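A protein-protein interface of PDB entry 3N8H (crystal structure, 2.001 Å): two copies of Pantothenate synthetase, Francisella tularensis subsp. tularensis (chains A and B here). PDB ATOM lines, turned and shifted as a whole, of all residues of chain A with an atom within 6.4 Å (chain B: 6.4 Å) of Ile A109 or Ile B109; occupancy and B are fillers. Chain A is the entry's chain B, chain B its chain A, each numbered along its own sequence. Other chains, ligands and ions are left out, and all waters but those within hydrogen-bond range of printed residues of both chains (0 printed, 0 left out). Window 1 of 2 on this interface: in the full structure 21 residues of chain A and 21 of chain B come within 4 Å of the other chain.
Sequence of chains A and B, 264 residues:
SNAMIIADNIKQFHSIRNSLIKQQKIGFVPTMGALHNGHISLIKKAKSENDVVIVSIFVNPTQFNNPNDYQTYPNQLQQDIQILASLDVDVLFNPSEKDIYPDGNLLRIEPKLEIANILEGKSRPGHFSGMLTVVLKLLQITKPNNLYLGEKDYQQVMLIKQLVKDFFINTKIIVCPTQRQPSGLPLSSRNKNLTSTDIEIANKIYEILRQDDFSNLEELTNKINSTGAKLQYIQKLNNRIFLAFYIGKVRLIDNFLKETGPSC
The backbone carbonyl oxygen of Ile A109 is in hydrogen-bond range of the side-chain hydroxyl of Ser A129 (2.8 Å).
The backbone NH (N) of Ile A109 is in hydrogen-bond range of the side-chain hydroxyl (OG1) of Thr A133 (2.7 Å).
The backbone NH of Ile B109 lies within hydrogen-bond range of the side-chain hydroxyl of Thr B133.
O of Ile B109 lies within hydrogen-bond range of OG of Ser B129, 2.8 Å away.
The side-chain carboxylate (OE1) of Glu A110 sits at hydrogen-bond distance from the side-chain hydroxyl (OG) of Ser A129 (3.5 Å).
The backbone carbonyl oxygen of Arg B108 lies close to the backbone carbonyl oxygen of Arg A108 (3.3 Å).
The backbone NH (N) of Glu B110 is in hydrogen-bond range of the backbone carbonyl oxygen (O) of Arg A108.
The backbone NH (N) of Glu A110 is in hydrogen-bond range of the backbone carbonyl oxygen (O) of Arg B108.
Ile A109 touches just these residues of chain B: Arg B108 (3.3 Å) and Ile B109 (3.2 Å).
Of chain A, only Arg A108 (3.4 Å) and Ile A109 (3.2 Å) come within 4 Å of Ile B109.
Printed residues of chain A within 4 Å of Glu B110: Leu A107, Arg A108 and Glu A110.
Of the printed residues of chain A, Phe B167 touches Leu A107 (3.7 Å) and Leu A136 (3.7 Å).
Printed residues of chain A within 4 Å of Leu B136: Leu A136 and Phe A167.
Printed residues of chain B within 4 Å of Leu A163: Leu B107 (3.4 Å).
Printed residues of chain A within 4 Å of Leu B107: Glu A110, Pro A111, Leu A163 and Phe A167.
Thr A133 touches none of the printed residues of chain B.
Ser B129 touches none of the printed residues of chain A.
Among the printed residues, 18 pairs touch across the chains.
Among the printed residues, no Asp or Glu carboxylate lies within 4 Å of a Lys or Arg side-chain nitrogen of the other chain.
Leu A107 touches Phe B167, and with the chains exchanged Phe A167 touches Leu B107.
Arg A108 touches Ile B109, and with the chains exchanged Ile A109 touches Arg B108.
Arg A108 touches Glu B110, and with the chains exchanged Glu A110 touches Arg B108.
Glu A110 touches its own counterpart, Glu B110.
13 positions are printed for both chains.
CA of Leu A107 touches O of Glu B110, 3.6 Å away.
CD1 of Leu A107 touches N of Leu B163 (3.4 Å).
O of Leu A107 touches CZ of Phe B167, at 3.7 Å.
Ile B109 touches Arg A108.
Arg B108 touches Ile A109.
CD1 of Ile B109 touches CD1 of Ile A109 (3.2 Å).
Glu B110 touches Glu A110.
Pro A111 touches Leu B107 (CA to CD2, 3.8 Å).
CA of Leu A163 touches CD1 of Leu B107 (3.4 Å).
CG of Leu B136 touches CD1 of Phe A167, 3.8 Å away.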
ATOM      1  N   LEU A 107      15.568 -16.345 -32.114  1.00  0.00           N
ATOM      2  CA  LEU A 107      14.462 -16.256 -31.163  1.00  0.00           C
ATOM      3  C   LEU A 107      14.777 -17.116 -29.947  1.00  0.00           C
ATOM      4  O   LEU A 107      14.883 -18.338 -30.048  1.00  0.00           O
ATOM      5  CB  LEU A 107      13.159 -16.719 -31.828  1.00  0.00           C
ATOM      6  CG  LEU A 107      12.815 -15.940 -33.104  1.00  0.00           C
ATOM      7  CD1 LEU A 107      11.529 -16.450 -33.743  1.00  0.00           C
ATOM      8  CD2 LEU A 107      12.724 -14.436 -32.817  1.00  0.00           C
ATOM      9  N   ARG A 108      14.923 -16.484 -28.795  1.00  0.00           N
ATOM     10  CA  ARG A 108      15.313 -17.208 -27.592  1.00  0.00           C
ATOM     11  C   ARG A 108      14.270 -17.092 -26.506  1.00  0.00           C
ATOM     12  O   ARG A 108      13.643 -16.048 -26.357  1.00  0.00           O
ATOM     13  CB  ARG A 108      16.611 -16.609 -27.085  1.00  0.00           C
ATOM     14  CG  ARG A 108      17.486 -16.200 -28.234  1.00  0.00           C
ATOM     15  CD  ARG A 108      18.809 -15.704 -27.754  1.00  0.00           C
ATOM     16  NE  ARG A 108      19.684 -15.390 -28.874  1.00  0.00           N
ATOM     17  CZ  ARG A 108      20.930 -14.968 -28.724  1.00  0.00           C
ATOM     18  NH1 ARG A 108      21.417 -14.803 -27.499  1.00  0.00           N
ATOM     19  NH2 ARG A 108      21.674 -14.690 -29.786  1.00  0.00           N
ATOM     20  N   ILE A 109      14.087 -18.163 -25.736  1.00  0.00           N
ATOM     21  CA  ILE A 109      13.335 -18.044 -24.500  1.00  0.00           C
ATOM     22  C   ILE A 109      14.210 -17.388 -23.433  1.00  0.00           C
ATOM     23  O   ILE A 109      15.288 -17.906 -23.118  1.00  0.00           O
ATOM     24  CB  ILE A 109      12.850 -19.404 -23.994  1.00  0.00           C
ATOM     25  CG1 ILE A 109      11.874 -20.033 -24.999  1.00  0.00           C
ATOM     26  CG2 ILE A 109      12.187 -19.234 -22.632  1.00  0.00           C
ATOM     27  CD1 ILE A 109      10.488 -19.372 -24.978  1.00  0.00           C
ATOM     28  N   GLU A 110      13.736 -16.270 -22.879  1.00  0.00           N
ATOM     29  CA  GLU A 110      14.434 -15.554 -21.805  1.00  0.00           C
ATOM     30  C   GLU A 110      13.675 -15.696 -20.478  1.00  0.00           C
ATOM     31  O   GLU A 110      12.555 -15.218 -20.351  1.00  0.00           O
ATOM     32  CB  GLU A 110      14.561 -14.076 -22.168  1.00  0.00           C
ATOM     33  CG  GLU A 110      15.557 -13.313 -21.315  1.00  0.00           C
ATOM     34  CD  GLU A 110      16.937 -13.964 -21.300  1.00  0.00           C
ATOM     35  OE1 GLU A 110      17.390 -14.457 -22.359  1.00  0.00           O
ATOM     36  OE2 GLU A 110      17.566 -13.979 -20.223  1.00  0.00           O
ATOM     37  N   PRO A 111      14.273 -16.376 -19.489  1.00  0.00           N
ATOM     38  CA  PRO A 111      13.616 -16.536 -18.196  1.00  0.00           C
ATOM     39  C   PRO A 111      13.797 -15.290 -17.318  1.00  0.00           C
ATOM     40  O   PRO A 111      14.908 -14.821 -17.088  1.00  0.00           O
ATOM     41  CB  PRO A 111      14.336 -17.745 -17.593  1.00  0.00           C
ATOM     42  CG  PRO A 111      15.729 -17.608 -18.146  1.00  0.00           C
ATOM     43  CD  PRO A 111      15.529 -17.137 -19.569  1.00  0.00           C
ATOM     44  N   PHE A 128      20.482 -20.948 -19.009  1.00  0.00           N
ATOM     45  CA  PHE A 128      19.060 -21.314 -18.895  1.00  0.00           C
ATOM     46  C   PHE A 128      18.237 -20.888 -20.131  1.00  0.00           C
ATOM     47  O   PHE A 128      17.340 -21.620 -20.573  1.00  0.00           O
ATOM     48  CB  PHE A 128      18.441 -20.757 -17.603  1.00  0.00           C
ATOM     49  CG  PHE A 128      18.772 -21.565 -16.362  1.00  0.00           C
ATOM     50  CD1 PHE A 128      18.930 -22.945 -16.431  1.00  0.00           C
ATOM     51  CD2 PHE A 128      18.928 -20.939 -15.136  1.00  0.00           C
ATOM     52  CE1 PHE A 128      19.238 -23.678 -15.296  1.00  0.00           C
ATOM     53  CE2 PHE A 128      19.230 -21.666 -14.000  1.00  0.00           C
ATOM     54  CZ  PHE A 128      19.382 -23.028 -14.070  1.00  0.00           C
ATOM     55  N   SER A 129      18.550 -19.714 -20.690  1.00  0.00           N
ATOM     56  CA  SER A 129      17.951 -19.302 -21.953  1.00  0.00           C
ATOM     57  C   SER A 129      18.206 -20.355 -23.055  1.00  0.00           C
ATOM     58  O   SER A 129      17.302 -20.741 -23.795  1.00  0.00           O
ATOM     59  CB  SER A 129      18.489 -17.931 -22.408  1.00  0.00           C
ATOM     60  OG  SER A 129      17.981 -17.601 -23.696  1.00  0.00           O
ATOM     61  N   GLY A 130      19.451 -20.778 -23.195  1.00  0.00           N
ATOM     62  CA  GLY A 130      19.790 -21.732 -24.236  1.00  0.00           C
ATOM     63  C   GLY A 130      19.117 -23.073 -24.041  1.00  0.00           C
ATOM     64  O   GLY A 130      18.705 -23.723 -25.014  1.00  0.00           O
ATOM     65  N   LEU A 132      16.288 -23.634 -22.230  1.00  0.00           N
ATOM     66  CA  LEU A 132      14.834 -23.481 -22.407  1.00  0.00           C
ATOM     67  C   LEU A 132      14.458 -23.385 -23.885  1.00  0.00           C
ATOM     68  O   LEU A 132      13.441 -23.930 -24.316  1.00  0.00           O
ATOM     69  CB  LEU A 132      14.335 -22.231 -21.665  1.00  0.00           C
ATOM     70  CG  LEU A 132      14.291 -22.414 -20.138  1.00  0.00           C
ATOM     71  CD1 LEU A 132      14.073 -21.076 -19.445  1.00  0.00           C
ATOM     72  CD2 LEU A 132      13.172 -23.407 -19.756  1.00  0.00           C
ATOM     73  N   THR A 133      15.287 -22.691 -24.662  1.00  0.00           N
ATOM     74  CA  THR A 133      15.012 -22.530 -26.080  1.00  0.00           C
ATOM     75  C   THR A 133      15.105 -23.902 -26.797  1.00  0.00           C
ATOM     76  O   THR A 133      14.261 -24.237 -27.618  1.00  0.00           O
ATOM     77  CB  THR A 133      15.963 -21.500 -26.722  1.00  0.00           C
ATOM     78  OG1 THR A 133      15.752 -20.217 -26.090  1.00  0.00           O
ATOM     79  CG2 THR A 133      15.688 -21.372 -28.216  1.00  0.00           C
ATOM     80  N   LEU A 136      12.161 -26.308 -25.614  1.00  0.00           N
ATOM     81  CA  LEU A 136      10.936 -25.920 -26.312  1.00  0.00           C
ATOM     82  C   LEU A 136      10.940 -26.470 -27.752  1.00  0.00           C
ATOM     83  O   LEU A 136       9.960 -27.025 -28.204  1.00  0.00           O
ATOM     84  CB  LEU A 136      10.761 -24.401 -26.306  1.00  0.00           C
ATOM     85  CG  LEU A 136       9.538 -23.923 -27.091  1.00  0.00           C
ATOM     86  CD1 LEU A 136       8.264 -24.614 -26.600  1.00  0.00           C
ATOM     87  CD2 LEU A 136       9.405 -22.389 -27.014  1.00  0.00           C
ATOM     88  N   LEU A 163       7.960 -23.730 -18.382  1.00  0.00           N
ATOM     89  CA  LEU A 163       7.895 -23.707 -19.836  1.00  0.00           C
ATOM     90  C   LEU A 163       6.686 -24.487 -20.380  1.00  0.00           C
ATOM     91  O   LEU A 163       5.950 -23.996 -21.220  1.00  0.00           O
ATOM     92  CB  LEU A 163       9.195 -24.267 -20.431  1.00  0.00           C
ATOM     93  CG  LEU A 163       9.257 -24.331 -21.955  1.00  0.00           C
ATOM     94  CD1 LEU A 163       9.695 -22.989 -22.563  1.00  0.00           C
ATOM     95  CD2 LEU A 163      10.179 -25.490 -22.407  1.00  0.00           C
ATOM     96  N   PHE A 167       3.571 -22.396 -22.273  1.00  0.00           N
ATOM     97  CA  PHE A 167       3.335 -22.539 -23.712  1.00  0.00           C
ATOM     98  C   PHE A 167       2.383 -23.651 -24.071  1.00  0.00           C
ATOM     99  O   PHE A 167       2.366 -24.128 -25.207  1.00  0.00           O
ATOM    100  CB  PHE A 167       4.658 -22.529 -24.505  1.00  0.00           C
ATOM    101  CG  PHE A 167       5.405 -21.235 -24.318  1.00  0.00           C
ATOM    102  CD1 PHE A 167       4.889 -20.057 -24.856  1.00  0.00           C
ATOM    103  CD2 PHE A 167       6.549 -21.167 -23.519  1.00  0.00           C
ATOM    104  CE1 PHE A 167       5.517 -18.834 -24.640  1.00  0.00           C
ATOM    105  CE2 PHE A 167       7.198 -19.945 -23.307  1.00  0.00           C
ATOM    106  CZ  PHE A 167       6.682 -18.780 -23.879  1.00  0.00           C
ATOM    107  N   LEU B 107       8.476 -16.170 -18.628  1.00  0.00           N
ATOM    108  CA  LEU B 107       9.256 -16.710 -19.761  1.00  0.00           C
ATOM    109  C   LEU B 107       8.873 -15.981 -21.042  1.00  0.00           C
ATOM    110  O   LEU B 107       7.698 -15.973 -21.436  1.00  0.00           O
ATOM    111  CB  LEU B 107       8.984 -18.209 -19.939  1.00  0.00           C
ATOM    112  CG  LEU B 107       9.330 -19.123 -18.763  1.00  0.00           C
ATOM    113  CD1 LEU B 107       8.943 -20.576 -19.117  1.00  0.00           C
ATOM    114  CD2 LEU B 107      10.795 -19.005 -18.388  1.00  0.00           C
ATOM    115  N   ARG B 108       9.855 -15.373 -21.691  1.00  0.00           N
ATOM    116  CA  ARG B 108       9.572 -14.485 -22.802  1.00  0.00           C
ATOM    117  C   ARG B 108      10.367 -14.893 -24.015  1.00  0.00           C
ATOM    118  O   ARG B 108      11.510 -15.338 -23.895  1.00  0.00           O
ATOM    119  CB  ARG B 108       9.960 -13.040 -22.442  1.00  0.00           C
ATOM    120  CG  ARG B 108       9.191 -12.470 -21.274  1.00  0.00           C
ATOM    121  CD  ARG B 108      10.015 -11.436 -20.587  1.00  0.00           C
ATOM    122  NE  ARG B 108       9.535 -11.180 -19.240  1.00  0.00           N
ATOM    123  CZ  ARG B 108       9.697 -10.023 -18.613  1.00  0.00           C
ATOM    124  NH1 ARG B 108      10.324  -9.025 -19.224  1.00  0.00           N
ATOM    125  NH2 ARG B 108       9.232  -9.862 -17.383  1.00  0.00           N
ATOM    126  N   ILE B 109       9.765 -14.714 -25.181  1.00  0.00           N
ATOM    127  CA  ILE B 109      10.486 -14.851 -26.433  1.00  0.00           C
ATOM    128  C   ILE B 109      11.218 -13.545 -26.689  1.00  0.00           C
ATOM    129  O   ILE B 109      10.599 -12.478 -26.703  1.00  0.00           O
ATOM    130  CB  ILE B 109       9.534 -15.131 -27.609  1.00  0.00           C
ATOM    131  CG1 ILE B 109       8.928 -16.528 -27.476  1.00  0.00           C
ATOM    132  CG2 ILE B 109      10.293 -15.039 -28.909  1.00  0.00           C
ATOM    133  CD1 ILE B 109       9.928 -17.635 -27.667  1.00  0.00           C
ATOM    134  N   GLU B 110      12.529 -13.639 -26.883  1.00  0.00           N
ATOM    135  CA  GLU B 110      13.390 -12.473 -27.072  1.00  0.00           C
ATOM    136  C   GLU B 110      13.955 -12.542 -28.479  1.00  0.00           C
ATOM    137  O   GLU B 110      14.633 -13.509 -28.822  1.00  0.00           O
ATOM    138  CB  GLU B 110      14.554 -12.555 -26.083  1.00  0.00           C
ATOM    139  CG  GLU B 110      15.172 -11.245 -25.686  1.00  0.00           C
ATOM    140  CD  GLU B 110      14.263 -10.413 -24.797  1.00  0.00           C
ATOM    141  OE1 GLU B 110      14.048 -10.789 -23.619  1.00  0.00           O
ATOM    142  OE2 GLU B 110      13.769  -9.376 -25.285  1.00  0.00           O
ATOM    143  N   PRO B 111      13.687 -11.523 -29.309  1.00  0.00           N
ATOM    144  CA  PRO B 111      14.206 -11.603 -30.659  1.00  0.00           C
ATOM    145  C   PRO B 111      15.620 -11.003 -30.747  1.00  0.00           C
ATOM    146  O   PRO B 111      15.852  -9.852 -30.393  1.00  0.00           O
ATOM    147  CB  PRO B 111      13.225 -10.742 -31.472  1.00  0.00           C
ATOM    148  CG  PRO B 111      12.425  -9.916 -30.442  1.00  0.00           C
ATOM    149  CD  PRO B 111      12.947 -10.275 -29.071  1.00  0.00           C
ATOM    150  N   PHE B 128       8.286  -6.108 -29.345  1.00  0.00           N
ATOM    151  CA  PHE B 128       8.318  -7.324 -30.179  1.00  0.00           C
ATOM    152  C   PHE B 128       8.433  -8.572 -29.311  1.00  0.00           C
ATOM    153  O   PHE B 128       7.929  -9.647 -29.677  1.00  0.00           O
ATOM    154  CB  PHE B 128       9.459  -7.268 -31.232  1.00  0.00           C
ATOM    155  CG  PHE B 128       9.123  -6.448 -32.474  1.00  0.00           C
ATOM    156  CD1 PHE B 128       7.814  -6.353 -32.934  1.00  0.00           C
ATOM    157  CD2 PHE B 128      10.126  -5.802 -33.193  1.00  0.00           C
ATOM    158  CE1 PHE B 128       7.492  -5.619 -34.078  1.00  0.00           C
ATOM    159  CE2 PHE B 128       9.816  -5.071 -34.336  1.00  0.00           C
ATOM    160  CZ  PHE B 128       8.492  -4.978 -34.774  1.00  0.00           C
ATOM    161  N   SER B 129       9.081  -8.428 -28.153  1.00  0.00           N
ATOM    162  CA  SER B 129       9.192  -9.539 -27.214  1.00  0.00           C
ATOM    163  C   SER B 129       7.794  -9.884 -26.693  1.00  0.00           C
ATOM    164  O   SER B 129       7.408 -11.049 -26.659  1.00  0.00           O
ATOM    165  CB  SER B 129      10.157  -9.211 -26.072  1.00  0.00           C
ATOM    166  OG  SER B 129      10.143 -10.212 -25.066  1.00  0.00           O
ATOM    167  N   GLY B 130       7.026  -8.866 -26.312  1.00  0.00           N
ATOM    168  CA  GLY B 130       5.667  -9.084 -25.838  1.00  0.00           C
ATOM    169  C   GLY B 130       4.766  -9.761 -26.856  1.00  0.00           C
ATOM    170  O   GLY B 130       4.003 -10.675 -26.520  1.00  0.00           O
ATOM    171  N   LEU B 132       5.598 -11.508 -29.713  1.00  0.00           N
ATOM    172  CA  LEU B 132       6.037 -12.879 -30.018  1.00  0.00           C
ATOM    173  C   LEU B 132       5.657 -13.899 -28.933  1.00  0.00           C
ATOM    174  O   LEU B 132       5.301 -15.034 -29.240  1.00  0.00           O
ATOM    175  CB  LEU B 132       7.551 -12.897 -30.226  1.00  0.00           C
ATOM    176  CG  LEU B 132       7.973 -12.260 -31.552  1.00  0.00           C
ATOM    177  CD1 LEU B 132       9.502 -12.116 -31.629  1.00  0.00           C
ATOM    178  CD2 LEU B 132       7.417 -13.096 -32.732  1.00  0.00           C
ATOM    179  N   THR B 133       5.744 -13.496 -27.667  1.00  0.00           N
ATOM    180  CA  THR B 133       5.396 -14.380 -26.557  1.00  0.00           C
ATOM    181  C   THR B 133       3.882 -14.702 -26.559  1.00  0.00           C
ATOM    182  O   THR B 133       3.474 -15.867 -26.483  1.00  0.00           O
ATOM    183  CB  THR B 133       5.803 -13.754 -25.194  1.00  0.00           C
ATOM    184  OG1 THR B 133       7.220 -13.479 -25.193  1.00  0.00           O
ATOM    185  CG2 THR B 133       5.478 -14.704 -24.053  1.00  0.00           C
ATOM    186  N   LEU B 136       3.012 -16.809 -29.753  1.00  0.00           N
ATOM    187  CA  LEU B 136       3.370 -18.205 -29.488  1.00  0.00           C
ATOM    188  C   LEU B 136       2.309 -18.897 -28.616  1.00  0.00           C
ATOM    189  O   LEU B 136       1.891 -20.009 -28.912  1.00  0.00           O
ATOM    190  CB  LEU B 136       4.752 -18.306 -28.821  1.00  0.00           C
ATOM    191  CG  LEU B 136       5.248 -19.749 -28.620  1.00  0.00           C
ATOM    192  CD1 LEU B 136       5.049 -20.612 -29.882  1.00  0.00           C
ATOM    193  CD2 LEU B 136       6.717 -19.787 -28.176  1.00  0.00           C
ATOM    194  N   LEU B 163       9.095 -17.106 -36.033  1.00  0.00           N
ATOM    195  CA  LEU B 163       8.554 -17.838 -34.879  1.00  0.00           C
ATOM    196  C   LEU B 163       7.958 -19.197 -35.247  1.00  0.00           C
ATOM    197  O   LEU B 163       8.173 -20.193 -34.563  1.00  0.00           O
ATOM    198  CB  LEU B 163       7.471 -17.010 -34.223  1.00  0.00           C
ATOM    199  CG  LEU B 163       6.872 -17.600 -32.954  1.00  0.00           C
ATOM    200  CD1 LEU B 163       7.806 -17.369 -31.754  1.00  0.00           C
ATOM    201  CD2 LEU B 163       5.432 -17.061 -32.697  1.00  0.00           C
ATOM    202  N   PHE B 167       9.874 -22.696 -34.037  1.00  0.00           N
ATOM    203  CA  PHE B 167       9.248 -23.552 -33.041  1.00  0.00           C
ATOM    204  C   PHE B 167       8.287 -24.542 -33.651  1.00  0.00           C
ATOM    205  O   PHE B 167       7.323 -24.979 -33.012  1.00  0.00           O
ATOM    206  CB  PHE B 167       8.629 -22.684 -31.940  1.00  0.00           C
ATOM    207  CG  PHE B 167       9.655 -21.814 -31.283  1.00  0.00           C
ATOM    208  CD1 PHE B 167      10.669 -22.396 -30.523  1.00  0.00           C
ATOM    209  CD2 PHE B 167       9.670 -20.447 -31.491  1.00  0.00           C
ATOM    210  CE1 PHE B 167      11.664 -21.619 -29.926  1.00  0.00           C
ATOM    211  CE2 PHE B 167      10.660 -19.650 -30.904  1.00  0.00           C
ATOM    212  CZ  PHE B 167      11.663 -20.232 -30.127  1.00  0.00           C
